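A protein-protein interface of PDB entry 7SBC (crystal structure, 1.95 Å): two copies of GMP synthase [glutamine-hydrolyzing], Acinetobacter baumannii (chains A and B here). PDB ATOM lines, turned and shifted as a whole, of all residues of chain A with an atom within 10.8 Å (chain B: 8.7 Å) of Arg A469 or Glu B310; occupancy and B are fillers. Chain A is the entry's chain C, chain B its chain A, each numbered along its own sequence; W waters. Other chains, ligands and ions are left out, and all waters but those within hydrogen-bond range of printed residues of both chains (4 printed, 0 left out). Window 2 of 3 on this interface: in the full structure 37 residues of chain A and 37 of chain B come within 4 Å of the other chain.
OE2 of Glu B310 is in salt-bridge range of NE of Arg A469 (3.7 Å).
The backbone carbonyl oxygen of Pro B524 lies within hydrogen-bond range of the backbone NH of Val A464.
The side-chain hydroxyl (OG1) of Thr B526 lies within hydrogen-bond range of the backbone carbonyl oxygen (O) of Val A462, 3.3 Å away.
O of Thr B526 sits at hydrogen-bond distance from NH1 of Arg A514 (2.9 Å).
O of Trp B529 is in hydrogen-bond range of N of Val A462 (2.8 Å).
The side-chain carboxylate (OD1) of Asp B308 sits at hydrogen-bond distance from the backbone NH (N) of Glu B310, at 2.8 Å.
NZ of Lys B312 lies within salt-bridge range of OE1 of Glu B530 (2.6 Å).
The guanidinium group of Arg B313 lies within salt-bridge range of the chain-end carboxylate of Glu B530 (2.7 Å).
The side-chain hydroxyl of Ser A461 is in hydrogen-bond range of the side-chain hydroxyl of Ser A513 (2.8 Å).
OG of Ser A461 is in hydrogen-bond range of NE of Arg A514.
O of Val A462 is in hydrogen-bond range of NH2 of Arg A514, 2.9 Å away.
Among the printed residues, pairs that only touch across the chains: Ser A461 with Trp B529 (3.3 Å), Gly A463 with Pro B524 (3.3 Å), Arg A514 with Trp B529 (3.4 Å), Tyr A471 with Pro B309 (3.6 Å), Val A462 with Glu B530 (3.8 Å) and Val A464 with Thr B526 (3.97 Å).
Of the printed residues of chain B, Val A462 touches Thr B526, Trp B529 and Glu B530.
No residue of chain B comes within 4 Å of Gly A468.
Lys A510 touches none of the printed residues of chain B.
Asp A511 touches none of the printed residues of chain B.
Of the printed residues of chain B, Arg A514 touches Thr B526 and Trp B529.
No residue of chain A comes within 4 Å of Asp B308.
Glu B310 touches one residue of chain A.
Ala B311 touches none of the printed residues of chain A.
No residue of chain A comes within 4 Å of Lys B314.
Printed residues of chain A within 4 Å of Pro B524: Gly A463 and Val A464.
The nearest printed residue of chain B that does not touch Ser A461 is Glu B530 (5.3 Å).
Of the 20 printed residues of chain B, 6 touch a printed residue of chain A.
Hydrophobic or aromatic side chains of chain B within 4 Å of the printed part of chain A: Pro B309, Pro B524 and Trp B529.
Along chain B the printed residues that touch a printed residue of chain A span positions 309 to 530.
Hydrophobic or aromatic side chains of chain A within 4 Å of the printed part of chain B: Val A462, Val A464 and Tyr A471.
Along chain A the printed residues that touch a printed residue of chain B span positions 461 to 514.
No position is printed for both chains.
Water W4 lies within hydrogen-bond range of OE2 of Glu B530, O of Lys A460 and OH of Tyr A471.
Water W3 lies within hydrogen-bond range of the side-chain hydroxyl of Tyr A471 (2.6 Å) and the backbone carbonyl oxygen of Thr B307 (2.9 Å).
Water W1 bridges the chain-end carboxylate (OXT) of Glu B530 (2.6 Å) and the guanidinium group (NH2) of Arg A469 (2.8 Å).
Water W2 bridges the backbone carbonyl oxygen (O) of Ser A513 (2.7 Å) and the backbone carbonyl oxygen (O) of Pro B524 (2.8 Å).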
ATOM      1  N   LYS A 460      -2.833   9.894 -23.861  1.00  0.00           N
ATOM      2  CA  LYS A 460      -4.255   9.594 -23.886  1.00  0.00           C
ATOM      3  C   LYS A 460      -5.000  10.602 -24.756  1.00  0.00           C
ATOM      4  O   LYS A 460      -4.521  11.705 -25.026  1.00  0.00           O
ATOM      5  CB  LYS A 460      -4.841   9.567 -22.461  1.00  0.00           C
ATOM      6  CG  LYS A 460      -4.268   8.432 -21.606  1.00  0.00           C
ATOM      7  CD  LYS A 460      -5.027   8.286 -20.296  1.00  0.00           C
ATOM      8  CE  LYS A 460      -4.444   7.160 -19.433  1.00  0.00           C
ATOM      9  NZ  LYS A 460      -5.212   7.039 -18.161  1.00  0.00           N
ATOM     10  N   SER A 461      -6.176  10.194 -25.220  1.00  0.00           N
ATOM     11  CA  SER A 461      -7.034  11.084 -25.990  1.00  0.00           C
ATOM     12  C   SER A 461      -8.478  10.697 -25.721  1.00  0.00           C
ATOM     13  O   SER A 461      -8.766   9.653 -25.135  1.00  0.00           O
ATOM     14  CB  SER A 461      -6.716  11.033 -27.500  1.00  0.00           C
ATOM     15  OG  SER A 461      -7.322   9.918 -28.132  1.00  0.00           O
ATOM     16  N   VAL A 462      -9.380  11.558 -26.162  1.00  0.00           N
ATOM     17  CA  VAL A 462     -10.804  11.401 -25.904  1.00  0.00           C
ATOM     18  C   VAL A 462     -11.422  10.481 -26.946  1.00  0.00           C
ATOM     19  O   VAL A 462     -11.042  10.494 -28.124  1.00  0.00           O
ATOM     20  CB  VAL A 462     -11.498  12.780 -25.899  1.00  0.00           C
ATOM     21  CG1 VAL A 462     -12.999  12.625 -25.784  1.00  0.00           C
ATOM     22  CG2 VAL A 462     -10.948  13.624 -24.770  1.00  0.00           C
ATOM     23  N   GLY A 463     -12.387   9.673 -26.507  1.00  0.00           N
ATOM     24  CA  GLY A 463     -13.255   8.965 -27.416  1.00  0.00           C
ATOM     25  C   GLY A 463     -14.699   9.105 -26.976  1.00  0.00           C
ATOM     26  O   GLY A 463     -14.992   9.505 -25.846  1.00  0.00           O
ATOM     27  N   VAL A 464     -15.603   8.781 -27.898  1.00  0.00           N
ATOM     28  CA  VAL A 464     -17.038   8.743 -27.626  1.00  0.00           C
ATOM     29  C   VAL A 464     -17.483   7.290 -27.666  1.00  0.00           C
ATOM     30  O   VAL A 464     -17.351   6.619 -28.698  1.00  0.00           O
ATOM     31  CB  VAL A 464     -17.847   9.591 -28.622  1.00  0.00           C
ATOM     32  CG1 VAL A 464     -18.029  10.994 -28.097  1.00  0.00           C
ATOM     33  CG2 VAL A 464     -17.179   9.601 -30.001  1.00  0.00           C
ATOM     34  N   VAL A 465     -18.003   6.808 -26.541  1.00  0.00           N
ATOM     35  CA  VAL A 465     -18.537   5.456 -26.435  1.00  0.00           C
ATOM     36  C   VAL A 465     -20.037   5.573 -26.195  1.00  0.00           C
ATOM     37  O   VAL A 465     -20.511   5.418 -25.064  1.00  0.00           O
ATOM     38  CB  VAL A 465     -17.844   4.666 -25.308  1.00  0.00           C
ATOM     39  CG1 VAL A 465     -18.230   3.191 -25.362  1.00  0.00           C
ATOM     40  CG2 VAL A 465     -16.332   4.834 -25.396  1.00  0.00           C
ATOM     41  N   GLY A 466     -20.787   5.863 -27.252  1.00  0.00           N
ATOM     42  CA  GLY A 466     -22.206   6.131 -27.083  1.00  0.00           C
ATOM     43  C   GLY A 466     -22.403   7.466 -26.393  1.00  0.00           C
ATOM     44  O   GLY A 466     -21.864   8.494 -26.820  1.00  0.00           O
ATOM     45  N   ASP A 467     -23.182   7.456 -25.309  1.00  0.00           N
ATOM     46  CA  ASP A 467     -23.376   8.644 -24.489  1.00  0.00           C
ATOM     47  C   ASP A 467     -22.210   8.906 -23.545  1.00  0.00           C
ATOM     48  O   ASP A 467     -22.179   9.965 -22.908  1.00  0.00           O
ATOM     49  CB  ASP A 467     -24.657   8.525 -23.656  1.00  0.00           C
ATOM     50  CG  ASP A 467     -25.884   8.200 -24.490  1.00  0.00           C
ATOM     51  OD1 ASP A 467     -26.173   8.958 -25.441  1.00  0.00           O
ATOM     52  OD2 ASP A 467     -26.565   7.188 -24.183  1.00  0.00           O
ATOM     53  N   GLY A 468     -21.266   7.970 -23.425  1.00  0.00           N
ATOM     54  CA  GLY A 468     -20.168   8.095 -22.494  1.00  0.00           C
ATOM     55  C   GLY A 468     -18.902   8.632 -23.136  1.00  0.00           C
ATOM     56  O   GLY A 468     -18.735   8.614 -24.354  1.00  0.00           O
ATOM     57  N   ARG A 469     -18.005   9.122 -22.286  1.00  0.00           N
ATOM     58  CA  ARG A 469     -16.721   9.667 -22.705  1.00  0.00           C
ATOM     59  C   ARG A 469     -15.615   8.702 -22.300  1.00  0.00           C
ATOM     60  O   ARG A 469     -15.597   8.217 -21.165  1.00  0.00           O
ATOM     61  CB  ARG A 469     -16.483  11.040 -22.074  1.00  0.00           C
ATOM     62  CG  ARG A 469     -15.081  11.605 -22.266  1.00  0.00           C
ATOM     63  CD  ARG A 469     -14.944  12.953 -21.545  1.00  0.00           C
ATOM     64  NE  ARG A 469     -13.693  13.649 -21.841  1.00  0.00           N
ATOM     65  CZ  ARG A 469     -12.585  13.541 -21.118  1.00  0.00           C
ATOM     66  NH1 ARG A 469     -12.518  12.734 -20.072  1.00  0.00           N
ATOM     67  NH2 ARG A 469     -11.521  14.269 -21.448  1.00  0.00           N
ATOM     68  N   ARG A 470     -14.711   8.418 -23.230  1.00  0.00           N
ATOM     69  CA  ARG A 470     -13.516   7.639 -22.954  1.00  0.00           C
ATOM     70  C   ARG A 470     -12.314   8.568 -22.933  1.00  0.00           C
ATOM     71  O   ARG A 470     -12.256   9.540 -23.693  1.00  0.00           O
ATOM     72  CB  ARG A 470     -13.311   6.543 -24.007  1.00  0.00           C
ATOM     73  CG  ARG A 470     -12.046   5.711 -23.799  1.00  0.00           C
ATOM     74  CD  ARG A 470     -11.949   4.549 -24.793  1.00  0.00           C
ATOM     75  NE  ARG A 470     -12.939   3.514 -24.523  1.00  0.00           N
ATOM     76  CZ  ARG A 470     -13.032   2.369 -25.190  1.00  0.00           C
ATOM     77  NH1 ARG A 470     -12.187   2.063 -26.165  1.00  0.00           N
ATOM     78  NH2 ARG A 470     -13.997   1.509 -24.872  1.00  0.00           N
ATOM     79  N   TYR A 471     -11.358   8.274 -22.055  1.00  0.00           N
ATOM     80  CA  TYR A 471     -10.066   8.961 -22.046  1.00  0.00           C
ATOM     81  C   TYR A 471      -9.017   7.880 -21.807  1.00  0.00           C
ATOM     82  O   TYR A 471      -8.847   7.417 -20.677  1.00  0.00           O
ATOM     83  CB  TYR A 471     -10.028  10.050 -20.978  1.00  0.00           C
ATOM     84  CG  TYR A 471      -8.763  10.875 -20.982  1.00  0.00           C
ATOM     85  CD1 TYR A 471      -8.368  11.568 -22.118  1.00  0.00           C
ATOM     86  CD2 TYR A 471      -7.966  10.970 -19.843  1.00  0.00           C
ATOM     87  CE1 TYR A 471      -7.206  12.321 -22.131  1.00  0.00           C
ATOM     88  CE2 TYR A 471      -6.806  11.725 -19.841  1.00  0.00           C
ATOM     89  CZ  TYR A 471      -6.432  12.404 -20.983  1.00  0.00           C
ATOM     90  OH  TYR A 471      -5.278  13.164 -20.979  1.00  0.00           O
ATOM     91  N   ALA A 472      -8.336   7.454 -22.869  1.00  0.00           N
ATOM     92  CA  ALA A 472      -7.540   6.235 -22.799  1.00  0.00           C
ATOM     93  C   ALA A 472      -6.370   6.322 -23.769  1.00  0.00           C
ATOM     94  O   ALA A 472      -6.232   7.278 -24.531  1.00  0.00           O
ATOM     95  CB  ALA A 472      -8.405   5.004 -23.079  1.00  0.00           C
ATOM     96  N   TRP A 473      -5.537   5.287 -23.748  1.00  0.00           N
ATOM     97  CA  TRP A 473      -4.263   5.303 -24.452  1.00  0.00           C
ATOM     98  C   TRP A 473      -4.446   5.362 -25.966  1.00  0.00           C
ATOM     99  O   TRP A 473      -5.481   4.978 -26.520  1.00  0.00           O
ATOM    100  CB  TRP A 473      -3.451   4.059 -24.094  1.00  0.00           C
ATOM    101  CG  TRP A 473      -3.300   3.847 -22.628  1.00  0.00           C
ATOM    102  CD1 TRP A 473      -3.874   2.858 -21.878  1.00  0.00           C
ATOM    103  CD2 TRP A 473      -2.521   4.636 -21.725  1.00  0.00           C
ATOM    104  NE1 TRP A 473      -3.496   2.980 -20.565  1.00  0.00           N
ATOM    105  CE2 TRP A 473      -2.670   4.068 -20.441  1.00  0.00           C
ATOM    106  CE3 TRP A 473      -1.713   5.765 -21.876  1.00  0.00           C
ATOM    107  CZ2 TRP A 473      -2.037   4.588 -19.315  1.00  0.00           C
ATOM    108  CZ3 TRP A 473      -1.083   6.282 -20.749  1.00  0.00           C
ATOM    109  CH2 TRP A 473      -1.249   5.692 -19.489  1.00  0.00           C
ATOM    110  N   LYS A 510     -10.959  -1.616 -24.108  1.00  0.00           N
ATOM    111  CA  LYS A 510     -11.487  -0.443 -23.414  1.00  0.00           C
ATOM    112  C   LYS A 510     -10.399   0.576 -23.111  1.00  0.00           C
ATOM    113  O   LYS A 510     -10.676   1.780 -23.030  1.00  0.00           O
ATOM    114  CB  LYS A 510     -12.173  -0.875 -22.116  1.00  0.00           C
ATOM    115  N   ASP A 511      -9.166   0.118 -22.953  1.00  0.00           N
ATOM    116  CA  ASP A 511      -8.043   0.964 -22.582  1.00  0.00           C
ATOM    117  C   ASP A 511      -7.415   1.701 -23.760  1.00  0.00           C
ATOM    118  O   ASP A 511      -6.369   2.337 -23.585  1.00  0.00           O
ATOM    119  CB  ASP A 511      -6.999   0.107 -21.873  1.00  0.00           C
ATOM    120  CG  ASP A 511      -7.558  -0.549 -20.629  1.00  0.00           C
ATOM    121  OD1 ASP A 511      -7.873   0.183 -19.667  1.00  0.00           O
ATOM    122  OD2 ASP A 511      -7.724  -1.785 -20.637  1.00  0.00           O
ATOM    123  N   VAL A 512      -8.012   1.640 -24.949  1.00  0.00           N
ATOM    124  CA  VAL A 512      -7.478   2.322 -26.120  1.00  0.00           C
ATOM    125  C   VAL A 512      -8.536   3.282 -26.648  1.00  0.00           C
ATOM    126  O   VAL A 512      -9.656   2.868 -26.973  1.00  0.00           O
ATOM    127  CB  VAL A 512      -7.032   1.334 -27.206  1.00  0.00           C
ATOM    128  CG1 VAL A 512      -6.582   2.087 -28.451  1.00  0.00           C
ATOM    129  CG2 VAL A 512      -5.905   0.447 -26.663  1.00  0.00           C
ATOM    130  N   SER A 513      -8.177   4.558 -26.741  1.00  0.00           N
ATOM    131  CA  SER A 513      -9.097   5.567 -27.255  1.00  0.00           C
ATOM    132  C   SER A 513      -8.993   5.754 -28.758  1.00  0.00           C
ATOM    133  O   SER A 513      -9.975   6.160 -29.394  1.00  0.00           O
ATOM    134  CB  SER A 513      -8.828   6.914 -26.590  1.00  0.00           C
ATOM    135  OG  SER A 513      -7.514   7.357 -26.910  1.00  0.00           O
ATOM    136  N   ARG A 514      -7.829   5.480 -29.336  1.00  0.00           N
ATOM    137  CA  ARG A 514      -7.519   5.991 -30.658  1.00  0.00           C
ATOM    138  C   ARG A 514      -6.348   5.207 -31.226  1.00  0.00           C
ATOM    139  O   ARG A 514      -5.481   4.741 -30.484  1.00  0.00           O
ATOM    140  CB  ARG A 514      -7.197   7.488 -30.584  1.00  0.00           C
ATOM    141  CG  ARG A 514      -6.989   8.180 -31.924  1.00  0.00           C
ATOM    142  CD  ARG A 514      -6.695   9.649 -31.715  1.00  0.00           C
ATOM    143  NE  ARG A 514      -7.698  10.278 -30.863  1.00  0.00           N
ATOM    144  CZ  ARG A 514      -8.716  11.001 -31.308  1.00  0.00           C
ATOM    145  NH1 ARG A 514      -8.890  11.226 -32.601  1.00  0.00           N
ATOM    146  NH2 ARG A 514      -9.573  11.520 -30.433  1.00  0.00           N
ATOM    147  N   LEU B 303      -2.029  27.699 -17.570  1.00  0.00           N
ATOM    148  CA  LEU B 303      -2.036  26.308 -18.004  1.00  0.00           C
ATOM    149  C   LEU B 303      -0.864  25.498 -17.461  1.00  0.00           C
ATOM    150  O   LEU B 303      -0.919  24.262 -17.487  1.00  0.00           O
ATOM    151  CB  LEU B 303      -2.032  26.239 -19.544  1.00  0.00           C
ATOM    152  CG  LEU B 303      -3.365  26.615 -20.187  1.00  0.00           C
ATOM    153  CD1 LEU B 303      -3.242  26.837 -21.708  1.00  0.00           C
ATOM    154  CD2 LEU B 303      -4.410  25.549 -19.874  1.00  0.00           C
ATOM    155  N   VAL B 306      -0.927  21.877 -15.632  1.00  0.00           N
ATOM    156  CA  VAL B 306      -2.286  21.357 -15.689  1.00  0.00           C
ATOM    157  C   VAL B 306      -2.336  20.309 -16.792  1.00  0.00           C
ATOM    158  O   VAL B 306      -2.141  20.630 -17.967  1.00  0.00           O
ATOM    159  CB  VAL B 306      -3.307  22.478 -15.941  1.00  0.00           C
ATOM    160  CG1 VAL B 306      -4.701  21.894 -16.191  1.00  0.00           C
ATOM    161  CG2 VAL B 306      -3.333  23.451 -14.746  1.00  0.00           C
ATOM    162  N   THR B 307      -2.604  19.054 -16.421  1.00  0.00           N
ATOM    163  CA  THR B 307      -2.616  17.970 -17.397  1.00  0.00           C
ATOM    164  C   THR B 307      -4.008  17.502 -17.801  1.00  0.00           C
ATOM    165  O   THR B 307      -4.149  16.919 -18.880  1.00  0.00           O
ATOM    166  CB  THR B 307      -1.822  16.763 -16.868  1.00  0.00           C
ATOM    167  OG1 THR B 307      -2.447  16.272 -15.676  1.00  0.00           O
ATOM    168  CG2 THR B 307      -0.391  17.177 -16.544  1.00  0.00           C
ATOM    169  N   ASP B 308      -5.028  17.736 -16.988  1.00  0.00           N
ATOM    170  CA  ASP B 308      -6.367  17.223 -17.303  1.00  0.00           C
ATOM    171  C   ASP B 308      -7.009  18.029 -18.432  1.00  0.00           C
ATOM    172  O   ASP B 308      -7.155  19.255 -18.298  1.00  0.00           O
ATOM    173  CB  ASP B 308      -7.226  17.265 -16.043  1.00  0.00           C
ATOM    174  CG  ASP B 308      -8.604  16.680 -16.250  1.00  0.00           C
ATOM    175  OD1 ASP B 308      -9.422  17.306 -16.940  1.00  0.00           O
ATOM    176  OD2 ASP B 308      -8.871  15.592 -15.711  1.00  0.00           O
ATOM    177  N   PRO B 309      -7.429  17.394 -19.539  1.00  0.00           N
ATOM    178  CA  PRO B 309      -7.980  18.167 -20.671  1.00  0.00           C
ATOM    179  C   PRO B 309      -9.239  18.942 -20.331  1.00  0.00           C
ATOM    180  O   PRO B 309      -9.473  20.014 -20.899  1.00  0.00           O
ATOM    181  CB  PRO B 309      -8.273  17.094 -21.731  1.00  0.00           C
ATOM    182  CG  PRO B 309      -7.525  15.895 -21.299  1.00  0.00           C
ATOM    183  CD  PRO B 309      -7.378  15.951 -19.825  1.00  0.00           C
ATOM    184  N   GLU B 310     -10.087  18.415 -19.450  1.00  0.00           N
ATOM    185  CA  GLU B 310     -11.281  19.171 -19.084  1.00  0.00           C
ATOM    186  C   GLU B 310     -10.909  20.399 -18.267  1.00  0.00           C
ATOM    187  O   GLU B 310     -11.488  21.477 -18.457  1.00  0.00           O
ATOM    188  CB  GLU B 310     -12.257  18.272 -18.334  1.00  0.00           C
ATOM    189  CG  GLU B 310     -12.608  17.039 -19.150  1.00  0.00           C
ATOM    190  CD  GLU B 310     -13.588  16.129 -18.460  1.00  0.00           C
ATOM    191  OE1 GLU B 310     -13.305  15.707 -17.318  1.00  0.00           O
ATOM    192  OE2 GLU B 310     -14.642  15.842 -19.063  1.00  0.00           O
ATOM    193  N   ALA B 311      -9.912  20.264 -17.395  1.00  0.00           N
ATOM    194  CA  ALA B 311      -9.422  21.423 -16.656  1.00  0.00           C
ATOM    195  C   ALA B 311      -8.778  22.437 -17.591  1.00  0.00           C
ATOM    196  O   ALA B 311      -8.948  23.647 -17.410  1.00  0.00           O
ATOM    197  CB  ALA B 311      -8.436  20.984 -15.574  1.00  0.00           C
ATOM    198  N   LYS B 312      -8.046  21.964 -18.606  1.00  0.00           N
ATOM    199  CA  LYS B 312      -7.450  22.886 -19.569  1.00  0.00           C
ATOM    200  C   LYS B 312      -8.522  23.675 -20.310  1.00  0.00           C
ATOM    201  O   LYS B 312      -8.418  24.901 -20.446  1.00  0.00           O
ATOM    202  CB  LYS B 312      -6.563  22.127 -20.558  1.00  0.00           C
ATOM    203  CG  LYS B 312      -5.322  21.511 -19.915  1.00  0.00           C
ATOM    204  CD  LYS B 312      -4.312  21.064 -20.988  1.00  0.00           C
ATOM    205  CE  LYS B 312      -4.980  20.327 -22.109  1.00  0.00           C
ATOM    206  NZ  LYS B 312      -3.975  19.849 -23.132  1.00  0.00           N
ATOM    207  N   ARG B 313      -9.575  22.992 -20.774  1.00  0.00           N
ATOM    208  CA  ARG B 313     -10.654  23.673 -21.484  1.00  0.00           C
ATOM    209  C   ARG B 313     -11.351  24.700 -20.589  1.00  0.00           C
ATOM    210  O   ARG B 313     -11.687  25.798 -21.039  1.00  0.00           O
ATOM    211  CB  ARG B 313     -11.662  22.650 -22.008  1.00  0.00           C
ATOM    212  CG  ARG B 313     -11.192  21.852 -23.240  1.00  0.00           C
ATOM    213  CD  ARG B 313     -12.209  20.778 -23.606  1.00  0.00           C
ATOM    214  NE  ARG B 313     -11.973  20.200 -24.929  1.00  0.00           N
ATOM    215  CZ  ARG B 313     -12.401  20.731 -26.068  1.00  0.00           C
ATOM    216  NH1 ARG B 313     -13.047  21.887 -26.092  1.00  0.00           N
ATOM    217  NH2 ARG B 313     -12.179  20.084 -27.212  1.00  0.00           N
ATOM    218  N   LYS B 314     -11.577  24.357 -19.323  1.00  0.00           N
ATOM    219  CA  LYS B 314     -12.204  25.308 -18.407  1.00  0.00           C
ATOM    220  C   LYS B 314     -11.314  26.523 -18.177  1.00  0.00           C
ATOM    221  O   LYS B 314     -11.795  27.664 -18.174  1.00  0.00           O
ATOM    222  CB  LYS B 314     -12.529  24.621 -17.081  1.00  0.00           C
ATOM    223  N   ILE B 315     -10.010  26.299 -17.998  1.00  0.00           N
ATOM    224  CA  ILE B 315      -9.079  27.398 -17.758  1.00  0.00           C
ATOM    225  C   ILE B 315      -9.039  28.344 -18.952  1.00  0.00           C
ATOM    226  O   ILE B 315      -9.104  29.569 -18.798  1.00  0.00           O
ATOM    227  CB  ILE B 315      -7.685  26.838 -17.423  1.00  0.00           C
ATOM    228  CG1 ILE B 315      -7.679  26.295 -15.994  1.00  0.00           C
ATOM    229  CG2 ILE B 315      -6.603  27.892 -17.611  1.00  0.00           C
ATOM    230  CD1 ILE B 315      -6.522  25.368 -15.716  1.00  0.00           C
ATOM    231  N   ILE B 316      -8.946  27.786 -20.164  1.00  0.00           N
ATOM    232  CA  ILE B 316      -8.831  28.602 -21.369  1.00  0.00           C
ATOM    233  C   ILE B 316     -10.101  29.407 -21.600  1.00  0.00           C
ATOM    234  O   ILE B 316     -10.042  30.592 -21.939  1.00  0.00           O
ATOM    235  CB  ILE B 316      -8.499  27.709 -22.581  1.00  0.00           C
ATOM    236  CG1 ILE B 316      -7.108  27.086 -22.397  1.00  0.00           C
ATOM    237  CG2 ILE B 316      -8.606  28.520 -23.874  1.00  0.00           C
ATOM    238  CD1 ILE B 316      -6.823  25.889 -23.317  1.00  0.00           C
ATOM    239  N   GLY B 317     -11.267  28.782 -21.416  1.00  0.00           N
ATOM    240  CA  GLY B 317     -12.512  29.509 -21.592  1.00  0.00           C
ATOM    241  C   GLY B 317     -12.671  30.621 -20.573  1.00  0.00           C
ATOM    242  O   GLY B 317     -13.131  31.719 -20.902  1.00  0.00           O
ATOM    243  N   PRO B 411     -10.570  26.441 -27.634  1.00  0.00           N
ATOM    244  CA  PRO B 411      -9.292  26.266 -26.921  1.00  0.00           C
ATOM    245  C   PRO B 411      -8.057  26.178 -27.811  1.00  0.00           C
ATOM    246  O   PRO B 411      -6.958  26.006 -27.266  1.00  0.00           O
ATOM    247  CB  PRO B 411      -9.469  24.942 -26.162  1.00  0.00           C
ATOM    248  CG  PRO B 411     -10.832  24.480 -26.398  1.00  0.00           C
ATOM    249  CD  PRO B 411     -11.495  25.315 -27.428  1.00  0.00           C
ATOM    250  N   GLY B 414      -4.579  24.377 -27.425  1.00  0.00           N
ATOM    251  CA  GLY B 414      -4.634  23.873 -26.066  1.00  0.00           C
ATOM    252  C   GLY B 414      -5.175  22.461 -25.975  1.00  0.00           C
ATOM    253  O   GLY B 414      -4.852  21.731 -25.031  1.00  0.00           O
ATOM    254  N   VAL B 415      -6.009  22.059 -26.939  1.00  0.00           N
ATOM    255  CA  VAL B 415      -6.517  20.693 -27.002  1.00  0.00           C
ATOM    256  C   VAL B 415      -5.812  19.873 -28.082  1.00  0.00           C
ATOM    257  O   VAL B 415      -6.264  18.772 -28.415  1.00  0.00           O
ATOM    258  CB  VAL B 415      -8.041  20.661 -27.192  1.00  0.00           C
ATOM    259  CG1 VAL B 415      -8.730  21.291 -25.987  1.00  0.00           C
ATOM    260  CG2 VAL B 415      -8.464  21.378 -28.489  1.00  0.00           C
ATOM    261  N   PRO B 524     -15.696   5.740 -33.015  1.00  0.00           N
ATOM    262  CA  PRO B 524     -15.703   6.086 -31.587  1.00  0.00           C
ATOM    263  C   PRO B 524     -14.593   7.038 -31.144  1.00  0.00           C
ATOM    264  O   PRO B 524     -14.408   7.238 -29.941  1.00  0.00           O
ATOM    265  CB  PRO B 524     -15.522   4.726 -30.917  1.00  0.00           C
ATOM    266  CG  PRO B 524     -14.612   3.998 -31.866  1.00  0.00           C
ATOM    267  CD  PRO B 524     -14.940   4.498 -33.261  1.00  0.00           C
ATOM    268  N   THR B 526     -13.164  10.995 -31.206  1.00  0.00           N
ATOM    269  CA  THR B 526     -13.576  12.356 -31.521  1.00  0.00           C
ATOM    270  C   THR B 526     -12.634  12.953 -32.567  1.00  0.00           C
ATOM    271  O   THR B 526     -11.565  12.414 -32.860  1.00  0.00           O
ATOM    272  CB  THR B 526     -13.601  13.237 -30.266  1.00  0.00           C
ATOM    273  OG1 THR B 526     -12.339  13.152 -29.588  1.00  0.00           O
ATOM    274  CG2 THR B 526     -14.721  12.808 -29.328  1.00  0.00           C
ATOM    275  N   TRP B 529      -8.422  15.609 -30.239  1.00  0.00           N
ATOM    276  CA  TRP B 529      -7.897  14.588 -29.334  1.00  0.00           C
ATOM    277  C   TRP B 529      -8.227  14.865 -27.870  1.00  0.00           C
ATOM    278  O   TRP B 529      -8.184  13.938 -27.051  1.00  0.00           O
ATOM    279  CB  TRP B 529      -6.383  14.479 -29.512  1.00  0.00           C
ATOM    280  CG  TRP B 529      -5.944  13.756 -30.771  1.00  0.00           C
ATOM    281  CD1 TRP B 529      -6.502  13.835 -32.022  1.00  0.00           C
ATOM    282  CD2 TRP B 529      -4.849  12.836 -30.881  1.00  0.00           C
ATOM    283  NE1 TRP B 529      -5.809  13.024 -32.904  1.00  0.00           N
ATOM    284  CE2 TRP B 529      -4.789  12.405 -32.225  1.00  0.00           C
ATOM    285  CE3 TRP B 529      -3.904  12.345 -29.971  1.00  0.00           C
ATOM    286  CZ2 TRP B 529      -3.829  11.488 -32.678  1.00  0.00           C
ATOM    287  CZ3 TRP B 529      -2.954  11.441 -30.421  1.00  0.00           C
ATOM    288  CH2 TRP B 529      -2.920  11.028 -31.768  1.00  0.00           C
ATOM    289  N   GLU B 530      -8.556  16.108 -27.529  1.00  0.00           N
ATOM    290  CA  GLU B 530      -8.914  16.483 -26.165  1.00  0.00           C
ATOM    291  C   GLU B 530     -10.137  17.392 -26.149  1.00  0.00           C
ATOM    292  O   GLU B 530     -10.616  17.840 -27.198  1.00  0.00           O
ATOM    293  CB  GLU B 530      -7.748  17.187 -25.466  1.00  0.00           C
ATOM    294  CG  GLU B 530      -6.580  16.279 -25.118  1.00  0.00           C
ATOM    295  CD  GLU B 530      -5.443  17.024 -24.429  1.00  0.00           C
ATOM    296  OE1 GLU B 530      -5.336  18.255 -24.636  1.00  0.00           O
ATOM    297  OE2 GLU B 530      -4.667  16.387 -23.674  1.00  0.00           O
ATOM    298  OXT GLU B 530     -10.657  17.703 -25.074  1.00  0.00           O
HETATM  299  O   HOH W   1     -11.674  16.720 -22.856  1.00  0.00           O
HETATM  300  O   HOH W   2     -12.532   5.766 -28.510  1.00  0.00           O
HETATM  301  O   HOH W   3      -3.626  14.105 -19.270  1.00  0.00           O
HETATM  302  O   HOH W   4      -4.348  13.935 -23.506  1.00  0.00           O
